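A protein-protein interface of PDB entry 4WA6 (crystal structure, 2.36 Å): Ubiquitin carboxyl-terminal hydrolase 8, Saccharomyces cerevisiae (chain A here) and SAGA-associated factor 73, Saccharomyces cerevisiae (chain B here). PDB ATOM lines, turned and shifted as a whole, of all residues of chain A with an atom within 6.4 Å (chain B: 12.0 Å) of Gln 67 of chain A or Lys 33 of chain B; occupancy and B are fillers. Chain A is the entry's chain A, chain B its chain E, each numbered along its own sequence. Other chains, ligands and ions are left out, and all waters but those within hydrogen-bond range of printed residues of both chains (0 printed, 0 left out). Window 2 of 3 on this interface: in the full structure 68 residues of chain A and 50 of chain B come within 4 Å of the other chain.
The side-chain amino group of Lys 33 of chain B lies within hydrogen-bond range of the backbone carbonyl oxygen of Leu 66 of chain A (3.3 Å).
NE1 of Trp 32 of chain B sits at hydrogen-bond distance from O of Cys 65 of chain A, at 2.7 Å.
The backbone carbonyl oxygen (O) of Cys 68 of chain A lies within hydrogen-bond range of the indole nitrogen (NE1) of Trp 32 of chain B (3.1 Å).
N of Trp 32 of chain B lies within hydrogen-bond range of O of Gly 69 of chain A (2.9 Å).
Thr 28 of chain A touches Trp 32 of chain B (CG2 to CZ2, 3.5 Å).
CB of Ala 31 of chain A touches CE of Met 36 of chain B (3.4 Å).
CD1 of Ile 35 of chain A touches O of Trp 32 of chain B, 3.6 Å away.
Leu 35 of chain B touches Ile 35 of chain A (CD1 to CG2, 3.5 Å).
CD1 of Ile 35 of chain A touches N of Met 36 of chain B, at 3.7 Å.
Met 64 of chain A touches Trp 32 of chain B (CE to CE3, 3.2 Å).
Gln 67 of chain A touches Lys 33 of chain B.
Cys 68 of chain A touches Lys 33 of chain B (O to CE, 3.6 Å).
Ser 31 of chain B touches Gly 69 of chain A.
O of Ser 31 of chain B is in hydrogen-bond range of OG of Ser 34 of chain B, at 2.9 Å.
N of Leu 66 of chain A sits at hydrogen-bond distance from O of Phe 90 of chain A (2.9 Å).
The backbone NH (N) of Lys 33 of chain B lies within hydrogen-bond range of the side-chain hydroxyl (OG) of Ser 31 of chain B (3.1 Å).
The side-chain sulfur (SG) of Cys 65 of chain A lies close to the backbone NH (N) of Gln 67 of chain A, 3.4 Å away.
Of the 13 printed residues of chain B, 5 touch a printed residue of chain A.
Hydrophobic or aromatic side chains of chain B within 4 Å of the printed part of chain A: Trp 32, Leu 35 and Met 36.
Along chain B the printed residues that touch a printed residue of chain A span positions 31 to 36.
Hydrophobic or aromatic side chains of chain A within 4 Å of the printed part of chain B: Ala 31, Ile 35 and Met 64.
Among the printed residues, no Asp or Glu carboxylate lies within 4 Å of a Lys or Arg side-chain nitrogen of the other chain.
Thr 28 of chain A touches just one residue of chain B: Trp 32 (3.5 Å).
Of the printed residues of chain B, Ile 35 of chain A touches Trp 32 (3.6 Å), Leu 35 (3.5 Å) and Met 36 (3.7 Å).
Printed residues of chain B within 4 Å of Met 64 of chain A: Trp 32 (3.2 Å).
Cys 65 of chain A touches just one residue of chain B: Trp 32.
Leu 66 of chain A touches just one residue of chain B: Lys 33.
Of the printed residues of chain B, Gln 67 of chain A touches Lys 33 (3.7 Å).
Gly 69 of chain A touches two residues of chain B.
No residue of chain B comes within 4 Å of His 88 of chain A.
No residue of chain B comes within 4 Å of Ile 89 of chain A.
No residue of chain B comes within 4 Å of Phe 90 of chain A.
Of the printed residues of chain A, Ser 31 of chain B touches Gly 69.
Lys 33 of chain B touches three residues of chain A.
Ser 34 of chain B touches none of the printed residues of chain A.
Of the printed residues of chain A, Leu 35 of chain B touches Ile 35.
Printed residues of chain A within 4 Å of Met 36 of chain B: Ala 31 and Ile 35.
The nearest residue of chain A that does not touch Lys 33 of chain B is Ile 35 of chain A (4.2 Å).
The nearest printed residue of chain A that does not touch Ser 31 of chain B is Cys 68 of chain A (5.3 Å).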
ATOM      1  N   THR A  28     -13.043  11.766 -22.800  1.00  0.00           N
ATOM      2  CA  THR A  28     -11.981  10.801 -22.566  1.00  0.00           C
ATOM      3  C   THR A  28     -11.416  10.897 -21.177  1.00  0.00           C
ATOM      4  O   THR A  28     -11.205   9.876 -20.572  1.00  0.00           O
ATOM      5  CB  THR A  28     -10.896  10.964 -23.619  1.00  0.00           C
ATOM      6  OG1 THR A  28     -11.537  10.967 -24.882  1.00  0.00           O
ATOM      7  CG2 THR A  28      -9.878   9.797 -23.546  1.00  0.00           C
ATOM      8  N   ALA A  31     -14.120   9.347 -18.783  1.00  0.00           N
ATOM      9  CA  ALA A  31     -14.195   7.905 -18.963  1.00  0.00           C
ATOM     10  C   ALA A  31     -12.974   7.208 -18.385  1.00  0.00           C
ATOM     11  O   ALA A  31     -13.080   6.191 -17.734  1.00  0.00           O
ATOM     12  CB  ALA A  31     -14.288   7.602 -20.437  1.00  0.00           C
ATOM     13  N   ILE A  35     -13.292   4.582 -15.503  1.00  0.00           N
ATOM     14  CA  ILE A  35     -12.723   3.250 -15.581  1.00  0.00           C
ATOM     15  C   ILE A  35     -11.778   2.935 -14.414  1.00  0.00           C
ATOM     16  O   ILE A  35     -11.779   1.804 -13.893  1.00  0.00           O
ATOM     17  CB  ILE A  35     -12.012   3.022 -16.906  1.00  0.00           C
ATOM     18  CG1 ILE A  35     -13.076   2.858 -17.991  1.00  0.00           C
ATOM     19  CG2 ILE A  35     -11.101   1.785 -16.804  1.00  0.00           C
ATOM     20  CD1 ILE A  35     -12.577   2.770 -19.416  1.00  0.00           C
ATOM     21  N   MET A  64      -2.474   6.184 -19.840  1.00  0.00           N
ATOM     22  CA  MET A  64      -3.508   5.736 -20.792  1.00  0.00           C
ATOM     23  C   MET A  64      -3.678   6.850 -21.823  1.00  0.00           C
ATOM     24  O   MET A  64      -4.029   7.949 -21.456  1.00  0.00           O
ATOM     25  CB  MET A  64      -4.838   5.513 -20.068  1.00  0.00           C
ATOM     26  CG  MET A  64      -4.908   4.369 -19.029  1.00  0.00           C
ATOM     27  SD  MET A  64      -6.153   4.652 -17.703  1.00  0.00           S
ATOM     28  CE  MET A  64      -7.608   4.107 -18.521  1.00  0.00           C
ATOM     29  N   CYS A  65      -3.425   6.580 -23.104  1.00  0.00           N
ATOM     30  CA  CYS A  65      -3.381   7.659 -24.079  1.00  0.00           C
ATOM     31  C   CYS A  65      -4.760   8.311 -24.216  1.00  0.00           C
ATOM     32  O   CYS A  65      -5.767   7.649 -24.111  1.00  0.00           O
ATOM     33  CB  CYS A  65      -2.855   7.193 -25.436  1.00  0.00           C
ATOM     34  SG  CYS A  65      -2.811   8.415 -26.769  1.00  0.00           S
ATOM     35  N   LEU A  66      -4.760   9.625 -24.434  1.00  0.00           N
ATOM     36  CA  LEU A  66      -5.961  10.385 -24.572  1.00  0.00           C
ATOM     37  C   LEU A  66      -6.590  10.184 -25.976  1.00  0.00           C
ATOM     38  O   LEU A  66      -7.803  10.132 -26.135  1.00  0.00           O
ATOM     39  CB  LEU A  66      -5.598  11.833 -24.363  1.00  0.00           C
ATOM     40  CG  LEU A  66      -6.596  12.724 -23.672  1.00  0.00           C
ATOM     41  CD1 LEU A  66      -6.792  12.220 -22.253  1.00  0.00           C
ATOM     42  CD2 LEU A  66      -6.094  14.166 -23.727  1.00  0.00           C
ATOM     43  N   GLN A  67      -5.766  10.019 -26.993  1.00  0.00           N
ATOM     44  CA  GLN A  67      -6.291   9.814 -28.318  1.00  0.00           C
ATOM     45  C   GLN A  67      -6.352   8.380 -28.843  1.00  0.00           C
ATOM     46  O   GLN A  67      -6.810   8.187 -29.938  1.00  0.00           O
ATOM     47  CB  GLN A  67      -5.491  10.663 -29.303  1.00  0.00           C
ATOM     48  CG  GLN A  67      -5.560  12.162 -29.008  1.00  0.00           C
ATOM     49  CD  GLN A  67      -4.320  12.860 -29.496  1.00  0.00           C
ATOM     50  OE1 GLN A  67      -3.269  12.789 -28.865  1.00  0.00           O
ATOM     51  NE2 GLN A  67      -4.418  13.508 -30.618  1.00  0.00           N
ATOM     52  N   CYS A  68      -5.893   7.378 -28.107  1.00  0.00           N
ATOM     53  CA  CYS A  68      -6.017   6.004 -28.583  1.00  0.00           C
ATOM     54  C   CYS A  68      -6.017   5.038 -27.384  1.00  0.00           C
ATOM     55  O   CYS A  68      -5.888   5.461 -26.238  1.00  0.00           O
ATOM     56  CB  CYS A  68      -4.921   5.695 -29.626  1.00  0.00           C
ATOM     57  SG  CYS A  68      -3.295   5.244 -28.962  1.00  0.00           S
ATOM     58  N   GLY A  69      -6.184   3.748 -27.621  1.00  0.00           N
ATOM     59  CA  GLY A  69      -6.266   2.827 -26.512  1.00  0.00           C
ATOM     60  C   GLY A  69      -4.953   2.426 -25.852  1.00  0.00           C
ATOM     61  O   GLY A  69      -4.977   1.728 -24.882  1.00  0.00           O
ATOM     62  N   GLY A  87       2.538  11.070 -32.348  1.00  0.00           N
ATOM     63  CA  GLY A  87       2.027  12.442 -32.213  1.00  0.00           C
ATOM     64  C   GLY A  87       0.987  12.587 -31.109  1.00  0.00           C
ATOM     65  O   GLY A  87       0.226  13.533 -31.114  1.00  0.00           O
ATOM     66  N   HIS A  88       0.942  11.662 -30.158  1.00  0.00           N
ATOM     67  CA  HIS A  88      -0.055  11.718 -29.084  1.00  0.00           C
ATOM     68  C   HIS A  88       0.634  12.071 -27.789  1.00  0.00           C
ATOM     69  O   HIS A  88       1.288  11.186 -27.173  1.00  0.00           O
ATOM     70  CB  HIS A  88      -0.743  10.386 -28.896  1.00  0.00           C
ATOM     71  CG  HIS A  88      -1.602   9.995 -30.041  1.00  0.00           C
ATOM     72  ND1 HIS A  88      -2.109   8.720 -30.191  1.00  0.00           N
ATOM     73  CD2 HIS A  88      -2.051  10.706 -31.099  1.00  0.00           C
ATOM     74  CE1 HIS A  88      -2.824   8.659 -31.298  1.00  0.00           C
ATOM     75  NE2 HIS A  88      -2.801   9.848 -31.869  1.00  0.00           N
ATOM     76  N   ILE A  89       0.457  13.325 -27.359  1.00  0.00           N
ATOM     77  CA  ILE A  89       1.310  13.873 -26.326  1.00  0.00           C
ATOM     78  C   ILE A  89       0.636  13.960 -24.958  1.00  0.00           C
ATOM     79  O   ILE A  89       1.241  14.485 -24.009  1.00  0.00           O
ATOM     80  CB  ILE A  89       1.914  15.242 -26.739  1.00  0.00           C
ATOM     81  CG1 ILE A  89       0.851  16.349 -26.667  1.00  0.00           C
ATOM     82  CG2 ILE A  89       2.525  15.136 -28.125  1.00  0.00           C
ATOM     83  CD1 ILE A  89       1.336  17.735 -27.051  1.00  0.00           C
ATOM     84  N   PHE A  90      -0.566  13.396 -24.841  1.00  0.00           N
ATOM     85  CA  PHE A  90      -1.287  13.369 -23.566  1.00  0.00           C
ATOM     86  C   PHE A  90      -1.753  11.981 -23.146  1.00  0.00           C
ATOM     87  O   PHE A  90      -2.366  11.233 -23.919  1.00  0.00           O
ATOM     88  CB  PHE A  90      -2.543  14.252 -23.651  1.00  0.00           C
ATOM     89  CG  PHE A  90      -2.306  15.612 -24.222  1.00  0.00           C
ATOM     90  CD1 PHE A  90      -1.651  16.572 -23.481  1.00  0.00           C
ATOM     91  CD2 PHE A  90      -2.762  15.935 -25.502  1.00  0.00           C
ATOM     92  CE1 PHE A  90      -1.439  17.840 -23.984  1.00  0.00           C
ATOM     93  CE2 PHE A  90      -2.592  17.221 -26.012  1.00  0.00           C
ATOM     94  CZ  PHE A  90      -1.919  18.178 -25.253  1.00  0.00           C
ATOM     95  N   ASP B  30      -5.149  -4.571 -27.972  1.00  0.00           N
ATOM     96  CA  ASP B  30      -6.393  -4.010 -27.468  1.00  0.00           C
ATOM     97  C   ASP B  30      -6.105  -2.695 -26.716  1.00  0.00           C
ATOM     98  O   ASP B  30      -5.005  -2.162 -26.820  1.00  0.00           O
ATOM     99  CB  ASP B  30      -7.180  -5.053 -26.634  1.00  0.00           C
ATOM    100  CG  ASP B  30      -6.303  -5.830 -25.659  1.00  0.00           C
ATOM    101  OD1 ASP B  30      -5.149  -5.428 -25.405  1.00  0.00           O
ATOM    102  OD2 ASP B  30      -6.781  -6.859 -25.150  1.00  0.00           O
ATOM    103  N   SER B  31      -7.081  -2.183 -25.965  1.00  0.00           N
ATOM    104  CA  SER B  31      -7.179  -0.760 -25.697  1.00  0.00           C
ATOM    105  C   SER B  31      -7.849  -0.447 -24.363  1.00  0.00           C
ATOM    106  O   SER B  31      -8.783  -1.128 -23.946  1.00  0.00           O
ATOM    107  CB  SER B  31      -8.004  -0.139 -26.805  1.00  0.00           C
ATOM    108  OG  SER B  31      -8.936   0.782 -26.291  1.00  0.00           O
ATOM    109  N   TRP B  32      -7.394   0.594 -23.687  1.00  0.00           N
ATOM    110  CA  TRP B  32      -7.956   0.905 -22.387  1.00  0.00           C
ATOM    111  C   TRP B  32      -9.436   1.325 -22.472  1.00  0.00           C
ATOM    112  O   TRP B  32     -10.151   1.128 -21.520  1.00  0.00           O
ATOM    113  CB  TRP B  32      -7.095   1.957 -21.652  1.00  0.00           C
ATOM    114  CG  TRP B  32      -7.185   3.390 -22.167  1.00  0.00           C
ATOM    115  CD1 TRP B  32      -6.270   4.037 -22.948  1.00  0.00           C
ATOM    116  CD2 TRP B  32      -8.226   4.341 -21.911  1.00  0.00           C
ATOM    117  NE1 TRP B  32      -6.671   5.323 -23.200  1.00  0.00           N
ATOM    118  CE2 TRP B  32      -7.867   5.539 -22.566  1.00  0.00           C
ATOM    119  CE3 TRP B  32      -9.424   4.304 -21.174  1.00  0.00           C
ATOM    120  CZ2 TRP B  32      -8.665   6.686 -22.515  1.00  0.00           C
ATOM    121  CZ3 TRP B  32     -10.224   5.433 -21.139  1.00  0.00           C
ATOM    122  CH2 TRP B  32      -9.843   6.614 -21.808  1.00  0.00           C
ATOM    123  N   LYS B  33      -9.909   1.869 -23.594  1.00  0.00           N
ATOM    124  CA  LYS B  33     -11.319   2.348 -23.681  1.00  0.00           C
ATOM    125  C   LYS B  33     -12.351   1.231 -23.635  1.00  0.00           C
ATOM    126  O   LYS B  33     -13.513   1.408 -23.223  1.00  0.00           O
ATOM    127  CB  LYS B  33     -11.552   3.232 -24.928  1.00  0.00           C
ATOM    128  CG  LYS B  33     -10.859   4.580 -24.809  1.00  0.00           C
ATOM    129  CD  LYS B  33     -10.591   5.289 -26.122  1.00  0.00           C
ATOM    130  CE  LYS B  33      -9.372   6.188 -25.953  1.00  0.00           C
ATOM    131  NZ  LYS B  33      -9.318   7.329 -26.882  1.00  0.00           N
ATOM    132  N   SER B  34     -11.910   0.056 -23.994  1.00  0.00           N
ATOM    133  CA  SER B  34     -12.774  -1.089 -24.016  1.00  0.00           C
ATOM    134  C   SER B  34     -13.052  -1.682 -22.637  1.00  0.00           C
ATOM    135  O   SER B  34     -13.684  -2.723 -22.554  1.00  0.00           O
ATOM    136  CB  SER B  34     -12.112  -2.161 -24.869  1.00  0.00           C
ATOM    137  OG  SER B  34     -11.133  -2.831 -24.080  1.00  0.00           O
ATOM    138  N   LEU B  35     -12.535  -1.092 -21.560  1.00  0.00           N
ATOM    139  CA  LEU B  35     -12.879  -1.541 -20.196  1.00  0.00           C
ATOM    140  C   LEU B  35     -14.226  -0.946 -19.750  1.00  0.00           C
ATOM    141  O   LEU B  35     -14.802  -1.325 -18.714  1.00  0.00           O
ATOM    142  CB  LEU B  35     -11.802  -1.092 -19.204  1.00  0.00           C
ATOM    143  CG  LEU B  35     -10.415  -1.737 -19.176  1.00  0.00           C
ATOM    144  CD1 LEU B  35      -9.417  -0.816 -18.489  1.00  0.00           C
ATOM    145  CD2 LEU B  35     -10.476  -3.061 -18.430  1.00  0.00           C
ATOM    146  N   MET B  36     -14.694   0.014 -20.532  1.00  0.00           N
ATOM    147  CA  MET B  36     -15.867   0.807 -20.186  1.00  0.00           C
ATOM    148  C   MET B  36     -17.118  -0.031 -19.966  1.00  0.00           C
ATOM    149  O   MET B  36     -17.853   0.256 -19.043  1.00  0.00           O
ATOM    150  CB  MET B  36     -16.139   1.872 -21.266  1.00  0.00           C
ATOM    151  CG  MET B  36     -17.277   2.815 -20.920  1.00  0.00           C
ATOM    152  SD  MET B  36     -17.234   3.589 -19.273  1.00  0.00           S
ATOM    153  CE  MET B  36     -15.980   4.871 -19.456  1.00  0.00           C
ATOM    154  N   SER B  37     -17.354  -1.047 -20.805  1.00  0.00           N
ATOM    155  CA  SER B  37     -18.514  -1.931 -20.641  1.00  0.00           C
ATOM    156  C   SER B  37     -18.445  -2.478 -19.255  1.00  0.00           C
ATOM    157  O   SER B  37     -19.330  -2.267 -18.451  1.00  0.00           O
ATOM    158  CB  SER B  37     -18.503  -3.082 -21.648  1.00  0.00           C
ATOM    159  OG  SER B  37     -19.217  -2.768 -22.841  1.00  0.00           O
ATOM    160  N   SER B  38     -17.349  -3.161 -18.958  1.00  0.00           N
ATOM    161  CA  SER B  38     -17.172  -3.774 -17.653  1.00  0.00           C
ATOM    162  C   SER B  38     -17.284  -2.797 -16.509  1.00  0.00           C
ATOM    163  O   SER B  38     -17.853  -3.118 -15.472  1.00  0.00           O
ATOM    164  CB  SER B  38     -15.802  -4.395 -17.563  1.00  0.00           C
ATOM    165  OG  SER B  38     -15.424  -4.422 -16.200  1.00  0.00           O
ATOM    166  N   ALA B  39     -16.672  -1.623 -16.664  1.00  0.00           N
ATOM    167  CA  ALA B  39     -16.634  -0.650 -15.579  1.00  0.00           C
ATOM    168  C   ALA B  39     -18.035  -0.186 -15.233  1.00  0.00           C
ATOM    169  O   ALA B  39     -18.366  -0.022 -14.055  1.00  0.00           O
ATOM    170  CB  ALA B  39     -15.759   0.536 -15.960  1.00  0.00           C
ATOM    171  N   LYS B  40     -18.851   0.018 -16.275  1.00  0.00           N
ATOM    172  CA  LYS B  40     -20.272   0.352 -16.125  1.00  0.00           C
ATOM    173  C   LYS B  40     -20.989  -0.630 -15.185  1.00  0.00           C
ATOM    174  O   LYS B  40     -21.845  -0.214 -14.402  1.00  0.00           O
ATOM    175  CB  LYS B  40     -20.974   0.366 -17.494  1.00  0.00           C
ATOM    176  CG  LYS B  40     -20.924   1.682 -18.273  1.00  0.00           C
ATOM    177  CD  LYS B  40     -21.857   1.583 -19.476  1.00  0.00           C
ATOM    178  CE  LYS B  40     -22.269   2.929 -20.073  1.00  0.00           C
ATOM    179  NZ  LYS B  40     -21.373   3.334 -21.201  1.00  0.00           N
ATOM    180  N   ASP B  41     -20.614  -1.911 -15.246  1.00  0.00           N
ATOM    181  CA  ASP B  41     -21.242  -2.967 -14.457  1.00  0.00           C
ATOM    182  C   ASP B  41     -20.385  -3.411 -13.264  1.00  0.00           C
ATOM    183  O   ASP B  41     -20.400  -4.583 -12.882  1.00  0.00           O
ATOM    184  CB  ASP B  41     -21.507  -4.172 -15.355  1.00  0.00           C
ATOM    185  CG  ASP B  41     -22.302  -5.257 -14.652  1.00  0.00           C
ATOM    186  OD1 ASP B  41     -23.522  -5.080 -14.486  1.00  0.00           O
ATOM    187  OD2 ASP B  41     -21.707  -6.292 -14.261  1.00  0.00           O
ATOM    188  N   THR B  42     -19.645  -2.480 -12.669  1.00  0.00           N
ATOM    189  CA  THR B  42     -18.694  -2.797 -11.603  1.00  0.00           C
ATOM    190  C   THR B  42     -18.772  -1.697 -10.533  1.00  0.00           C
ATOM    191  O   THR B  42     -18.682  -0.496 -10.837  1.00  0.00           O
ATOM    192  CB  THR B  42     -17.276  -2.862 -12.184  1.00  0.00           C
ATOM    193  OG1 THR B  42     -17.295  -3.608 -13.397  1.00  0.00           O
ATOM    194  CG2 THR B  42     -16.279  -3.487 -11.243  1.00  0.00           C
